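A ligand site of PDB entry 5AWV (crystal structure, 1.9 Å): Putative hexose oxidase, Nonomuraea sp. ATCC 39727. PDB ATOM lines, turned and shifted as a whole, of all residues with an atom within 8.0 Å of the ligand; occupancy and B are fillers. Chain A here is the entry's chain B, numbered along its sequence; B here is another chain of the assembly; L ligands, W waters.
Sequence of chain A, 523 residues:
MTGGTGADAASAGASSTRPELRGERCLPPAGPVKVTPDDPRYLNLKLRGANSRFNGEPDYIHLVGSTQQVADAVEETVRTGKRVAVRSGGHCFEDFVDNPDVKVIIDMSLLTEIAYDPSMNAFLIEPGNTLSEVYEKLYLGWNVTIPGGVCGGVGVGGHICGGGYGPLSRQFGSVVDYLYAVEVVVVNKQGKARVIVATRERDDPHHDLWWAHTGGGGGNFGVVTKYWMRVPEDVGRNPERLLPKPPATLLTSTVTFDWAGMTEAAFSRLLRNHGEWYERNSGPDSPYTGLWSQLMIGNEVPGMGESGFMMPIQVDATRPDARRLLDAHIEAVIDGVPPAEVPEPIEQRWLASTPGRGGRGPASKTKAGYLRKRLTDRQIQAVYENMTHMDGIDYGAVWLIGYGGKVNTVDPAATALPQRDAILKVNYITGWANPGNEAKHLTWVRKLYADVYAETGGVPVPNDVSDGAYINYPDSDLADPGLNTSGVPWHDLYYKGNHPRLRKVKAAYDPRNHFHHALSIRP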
ATOM      1  N   TRP A 432     -11.255  27.746 -13.511  1.00  0.00           N
ATOM      2  CA  TRP A 432     -10.942  29.173 -13.576  1.00  0.00           C
ATOM      3  C   TRP A 432     -12.081  29.927 -14.231  1.00  0.00           C
ATOM      4  O   TRP A 432     -12.745  29.425 -15.112  1.00  0.00           O
ATOM      5  CB  TRP A 432      -9.631  29.449 -14.302  1.00  0.00           C
ATOM      6  CG  TRP A 432      -9.482  28.914 -15.667  1.00  0.00           C
ATOM      7  CD1 TRP A 432      -9.602  29.599 -16.826  1.00  0.00           C
ATOM      8  CD2 TRP A 432      -9.083  27.594 -16.032  1.00  0.00           C
ATOM      9  NE1 TRP A 432      -9.372  28.785 -17.891  1.00  0.00           N
ATOM     10  CE2 TRP A 432      -9.040  27.549 -17.427  1.00  0.00           C
ATOM     11  CE3 TRP A 432      -8.861  26.424 -15.321  1.00  0.00           C
ATOM     12  CZ2 TRP A 432      -8.789  26.390 -18.108  1.00  0.00           C
ATOM     13  CZ3 TRP A 432      -8.534  25.281 -16.010  1.00  0.00           C
ATOM     14  CH2 TRP A 432      -8.488  25.259 -17.350  1.00  0.00           C
ATOM     15  N   ASN A 434     -11.775  33.348 -15.521  1.00  0.00           N
ATOM     16  CA  ASN A 434     -11.347  34.178 -16.641  1.00  0.00           C
ATOM     17  C   ASN A 434     -10.313  33.420 -17.500  1.00  0.00           C
ATOM     18  O   ASN A 434      -9.239  33.078 -16.964  1.00  0.00           O
ATOM     19  CB  ASN A 434     -10.750  35.428 -15.996  1.00  0.00           C
ATOM     20  CG  ASN A 434      -9.962  36.312 -16.948  1.00  0.00           C
ATOM     21  OD1 ASN A 434      -9.989  36.211 -18.180  1.00  0.00           O
ATOM     22  ND2 ASN A 434      -9.221  37.198 -16.341  1.00  0.00           N
ATOM     23  N   PRO A 435     -10.566  33.253 -18.810  1.00  0.00           N
ATOM     24  CA  PRO A 435      -9.658  32.617 -19.789  1.00  0.00           C
ATOM     25  C   PRO A 435      -8.207  33.100 -19.728  1.00  0.00           C
ATOM     26  O   PRO A 435      -7.269  32.311 -19.903  1.00  0.00           O
ATOM     27  CB  PRO A 435     -10.272  32.973 -21.150  1.00  0.00           C
ATOM     28  CG  PRO A 435     -11.700  33.227 -20.832  1.00  0.00           C
ATOM     29  CD  PRO A 435     -11.734  33.851 -19.504  1.00  0.00           C
ATOM     30  N   GLY A 436      -8.009  34.356 -19.382  1.00  0.00           N
ATOM     31  CA  GLY A 436      -6.689  34.854 -19.137  1.00  0.00           C
ATOM     32  C   GLY A 436      -5.854  34.155 -18.088  1.00  0.00           C
ATOM     33  O   GLY A 436      -4.650  34.221 -18.148  1.00  0.00           O
ATOM     34  N   ASN A 437      -6.477  33.517 -17.130  1.00  0.00           N
ATOM     35  CA  ASN A 437      -5.785  32.789 -16.077  1.00  0.00           C
ATOM     36  C   ASN A 437      -5.646  31.278 -16.317  1.00  0.00           C
ATOM     37  O   ASN A 437      -5.248  30.540 -15.418  1.00  0.00           O
ATOM     38  CB  ASN A 437      -6.559  32.951 -14.772  1.00  0.00           C
ATOM     39  CG  ASN A 437      -6.463  34.358 -14.229  1.00  0.00           C
ATOM     40  OD1 ASN A 437      -7.327  34.758 -13.463  1.00  0.00           O
ATOM     41  ND2 ASN A 437      -5.437  35.116 -14.623  1.00  0.00           N
ATOM     42  N   GLU A 438      -5.963  30.837 -17.507  1.00  0.00           N
ATOM     43  CA  GLU A 438      -5.825  29.408 -17.874  1.00  0.00           C
ATOM     44  C   GLU A 438      -4.422  28.848 -17.575  1.00  0.00           C
ATOM     45  O   GLU A 438      -4.293  27.822 -16.942  1.00  0.00           O
ATOM     46  CB  GLU A 438      -6.113  29.226 -19.357  1.00  0.00           C
ATOM     47  CG  GLU A 438      -5.925  27.785 -19.802  1.00  0.00           C
ATOM     48  CD  GLU A 438      -6.154  27.520 -21.290  1.00  0.00           C
ATOM     49  OE1 GLU A 438      -7.259  27.087 -21.643  1.00  0.00           O
ATOM     50  OE2 GLU A 438      -5.239  27.701 -22.129  1.00  0.00           O
ATOM     51  N   ALA A 439      -3.358  29.536 -18.017  1.00  0.00           N
ATOM     52  CA  ALA A 439      -2.006  28.931 -17.964  1.00  0.00           C
ATOM     53  C   ALA A 439      -1.600  28.633 -16.542  1.00  0.00           C
ATOM     54  O   ALA A 439      -1.036  27.577 -16.225  1.00  0.00           O
ATOM     55  CB  ALA A 439      -0.989  29.858 -18.669  1.00  0.00           C
ATOM     56  N   LYS A 440      -1.957  29.542 -15.629  1.00  0.00           N
ATOM     57  CA  LYS A 440      -1.591  29.391 -14.192  1.00  0.00           C
ATOM     58  C   LYS A 440      -2.269  28.212 -13.563  1.00  0.00           C
ATOM     59  O   LYS A 440      -1.692  27.537 -12.715  1.00  0.00           O
ATOM     60  CB  LYS A 440      -2.026  30.663 -13.396  1.00  0.00           C
ATOM     61  CG  LYS A 440      -1.022  31.156 -12.357  1.00  0.00           C
ATOM     62  CD  LYS A 440      -0.681  32.664 -12.472  1.00  0.00           C
ATOM     63  CE  LYS A 440      -1.915  33.550 -12.560  1.00  0.00           C
ATOM     64  NZ  LYS A 440      -3.018  33.146 -11.625  1.00  0.00           N
ATOM     65  N   HIS A 441      -3.532  28.009 -13.937  1.00  0.00           N
ATOM     66  CA  HIS A 441      -4.340  26.925 -13.388  1.00  0.00           C
ATOM     67  C   HIS A 441      -3.878  25.566 -13.923  1.00  0.00           C
ATOM     68  O   HIS A 441      -3.777  24.645 -13.155  1.00  0.00           O
ATOM     69  CB  HIS A 441      -5.811  27.117 -13.646  1.00  0.00           C
ATOM     70  CG  HIS A 441      -6.443  28.159 -12.810  1.00  0.00           C
ATOM     71  ND1 HIS A 441      -6.286  29.514 -13.049  1.00  0.00           N
ATOM     72  CD2 HIS A 441      -7.317  28.045 -11.784  1.00  0.00           C
ATOM     73  CE1 HIS A 441      -6.984  30.184 -12.151  1.00  0.00           C
ATOM     74  NE2 HIS A 441      -7.621  29.316 -11.384  1.00  0.00           N
ATOM     75  N   LEU A 442      -3.603  25.474 -15.196  1.00  0.00           N
ATOM     76  CA  LEU A 442      -3.022  24.239 -15.817  1.00  0.00           C
ATOM     77  C   LEU A 442      -1.681  23.910 -15.187  1.00  0.00           C
ATOM     78  O   LEU A 442      -1.433  22.775 -14.781  1.00  0.00           O
ATOM     79  CB  LEU A 442      -2.829  24.396 -17.314  1.00  0.00           C
ATOM     80  CG  LEU A 442      -4.060  24.575 -18.164  1.00  0.00           C
ATOM     81  CD1 LEU A 442      -3.733  24.710 -19.628  1.00  0.00           C
ATOM     82  CD2 LEU A 442      -5.004  23.365 -17.937  1.00  0.00           C
ATOM     83  N   3FG B   3       3.442  30.800 -14.731  1.00  0.00           N
ATOM     84  OD1 3FG B   3       1.896  33.536 -19.719  1.00  0.00           O
ATOM     85  CD1 3FG B   3       2.071  33.485 -18.374  1.00  0.00           C
ATOM     86  CG1 3FG B   3       2.094  32.213 -17.777  1.00  0.00           C
ATOM     87  CZ  3FG B   3       2.260  34.658 -17.633  1.00  0.00           C
ATOM     88  CD2 3FG B   3       2.443  34.540 -16.237  1.00  0.00           C
ATOM     89  OD2 3FG B   3       2.630  35.711 -15.510  1.00  0.00           O
ATOM     90  CG2 3FG B   3       2.428  33.247 -15.646  1.00  0.00           C
ATOM     91  CB  3FG B   3       2.274  32.056 -16.397  1.00  0.00           C
ATOM     92  CA  3FG B   3       2.293  30.765 -15.702  1.00  0.00           C
ATOM     93  C   3FG B   3       2.346  29.600 -16.540  1.00  0.00           C
ATOM     94  O   3FG B   3       1.341  28.866 -16.643  1.00  0.00           O
ATOM     95  N   GHP B   4       3.534  29.309 -17.299  1.00  0.00           N
ATOM     96  CA  GHP B   4       3.596  28.072 -18.150  1.00  0.00           C
ATOM     97  C   GHP B   4       2.881  28.266 -19.365  1.00  0.00           C
ATOM     98  O   GHP B   4       2.993  29.273 -20.041  1.00  0.00           O
ATOM     99  C1  GHP B   4       4.967  27.544 -18.386  1.00  0.00           C
ATOM    100  C2  GHP B   4       5.423  26.957 -19.590  1.00  0.00           C
ATOM    101  C3  GHP B   4       6.757  26.474 -19.710  1.00  0.00           C
ATOM    102  C4  GHP B   4       7.604  26.526 -18.593  1.00  0.00           C
ATOM    103  O4  GHP B   4       8.898  26.036 -18.684  1.00  0.00           O
ATOM    104  C5  GHP B   4       7.229  27.116 -17.416  1.00  0.00           C
ATOM    105  C6  GHP B   4       5.897  27.585 -17.331  1.00  0.00           C
ATOM    106  N   GHP B   5       2.181  27.155 -19.883  1.00  0.00           N
ATOM    107  CA  GHP B   5       1.726  27.117 -21.266  1.00  0.00           C
ATOM    108  C   GHP B   5       1.731  25.736 -21.720  1.00  0.00           C
ATOM    109  O   GHP B   5       1.579  24.776 -20.965  1.00  0.00           O
ATOM    110  C1  GHP B   5       0.469  27.643 -21.662  1.00  0.00           C
ATOM    111  C2  GHP B   5       0.446  28.536 -22.763  1.00  0.00           C
ATOM    112  C3  GHP B   5      -0.772  29.035 -23.299  1.00  0.00           C
ATOM    113  C4  GHP B   5      -1.941  28.654 -22.623  1.00  0.00           C
ATOM    114  O4  GHP B   5      -3.053  29.188 -23.137  1.00  0.00           O
ATOM    115  C5  GHP B   5      -1.927  27.770 -21.529  1.00  0.00           C
ATOM    116  C6  GHP B   5      -0.723  27.232 -21.022  1.00  0.00           C
ATOM    117  N   OMY B   6       1.935  25.422 -23.059  1.00  0.00           N
ATOM    118  CA  OMY B   6       2.310  26.266 -24.223  1.00  0.00           C
ATOM    119  OCZ OMY B   6       7.300  25.870 -20.846  1.00  0.00           O
ATOM    120  CE2 OMY B   6       5.661  24.514 -22.000  1.00  0.00           C
ATOM    121  CE1 OMY B   6       6.119  26.747 -22.696  1.00  0.00           C
ATOM    122  CZ  OMY B   6       6.374  25.680 -21.860  1.00  0.00           C
ATOM    123  CG  OMY B   6       4.473  25.502 -23.907  1.00  0.00           C
ATOM    124  CD2 OMY B   6       4.712  24.426 -23.017  1.00  0.00           C
ATOM    125  CD1 OMY B   6       5.167  26.689 -23.716  1.00  0.00           C
ATOM    126  CB  OMY B   6       3.424  25.459 -24.900  1.00  0.00           C
ATOM    127 CL   OMY B   6       7.021  28.218 -22.396  1.00  0.00          CL
ATOM    128  O   OMY B   6       0.102  25.668 -24.836  1.00  0.00           O
ATOM    129  C   OMY B   6       1.138  26.531 -24.958  1.00  0.00           C
ATOM    130  ODE OMY B   6       2.771  24.179 -24.969  1.00  0.00           O
ATOM    131  N   3FG B   7       0.976  27.684 -25.553  1.00  0.00           N
ATOM    132  OD1 3FG B   7      -1.070  31.655 -22.897  1.00  0.00           O
ATOM    133  CD1 3FG B   7      -0.847  31.320 -24.201  1.00  0.00           C
ATOM    134  CG1 3FG B   7      -0.713  29.931 -24.428  1.00  0.00           C
ATOM    135  CZ  3FG B   7      -0.714  32.262 -25.254  1.00  0.00           C
ATOM    136  CD2 3FG B   7      -0.454  31.819 -26.519  1.00  0.00           C
ATOM    137  OD2 3FG B   7      -0.371  32.710 -27.514  1.00  0.00           O
ATOM    138  CG2 3FG B   7      -0.308  30.451 -26.780  1.00  0.00           C
ATOM    139  CB  3FG B   7      -0.429  29.492 -25.763  1.00  0.00           C
ATOM    140  CA  3FG B   7      -0.310  28.096 -26.095  1.00  0.00           C
ATOM    141  C   3FG B   7      -0.536  27.796 -27.485  1.00  0.00           C
ATOM    142  O   3FG B   7      -1.720  27.970 -27.916  1.00  0.00           O
ATOM    143  OXT 3FG B   7       0.421  27.352 -28.151  1.00  0.00           O
HETATM  144  C1  LIG L   1      -1.538  32.938 -22.589  1.00  0.00           C
HETATM  145  C2  LIG L   1      -1.860  32.882 -21.094  1.00  0.00           C
HETATM  146  C3  LIG L   1      -3.179  32.119 -20.862  1.00  0.00           C
HETATM  147  C4  LIG L   1      -4.340  32.715 -21.767  1.00  0.00           C
HETATM  148  C5  LIG L   1      -3.929  32.718 -23.269  1.00  0.00           C
HETATM  149  C6  LIG L   1      -4.935  33.448 -24.151  1.00  0.00           C
HETATM  150  O1  LIG L   1      -1.906  34.225 -20.534  1.00  0.00           O
HETATM  151  O2  LIG L   1      -3.444  32.062 -19.412  1.00  0.00           O
HETATM  152  O3  LIG L   1      -5.518  31.904 -21.645  1.00  0.00           O
HETATM  153  O4  LIG L   1      -2.665  33.351 -23.473  1.00  0.00           O
HETATM  154  O5  LIG L   1      -4.821  34.815 -23.721  1.00  0.00           O
HETATM  155  O   HOH W   1      -2.370  32.391 -16.404  1.00  0.00           O
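The backbone NH of Ala 439 is in hydrogen-bond range of an oxygen (O2) of the ligand (2.9 Å).
The backbone carbonyl oxygen of Pro 435 sits at hydrogen-bond distance from an oxygen (O3) of the ligand, 2.5 Å away.
OD1 of 3FG 7 of chain B is bonded to C1 of the ligand (1.4 Å).
O2 of the ligand is in hydrogen-bond range of O of Gly 436, at 2.8 Å.
N of Glu 438 is in hydrogen-bond range of O2 of the ligand (3.4 Å).
O of 3FG 3 of chain B sits close to the backbone carbonyl oxygen (O) of Ala 439, 2.7 Å away.
A ring nitrogen (ND1) of His 441 is in hydrogen-bond range of the backbone carbonyl oxygen of Asn 437.
O4 of GHP 5 of chain B is in hydrogen-bond range of the side-chain carboxylate (OE2) of Glu 438 (2.8 Å).
OD1 of Asn 434 is in hydrogen-bond range of N of Gly 436 (3.0 Å).
CG1 of 3FG 7 of chain B is bonded to C3 of GHP 5 of chain B.
Merely in contact with the ligand: Asn 437, 3FG 3 of chain B and GHP 5 of chain B.
Water W1 lies within hydrogen-bond range of N of Lys 440 (3.0 Å), O2 of the ligand (3.2 Å), O of Gly 436 (3.4 Å) and N of Ala 439 (3.4 Å).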
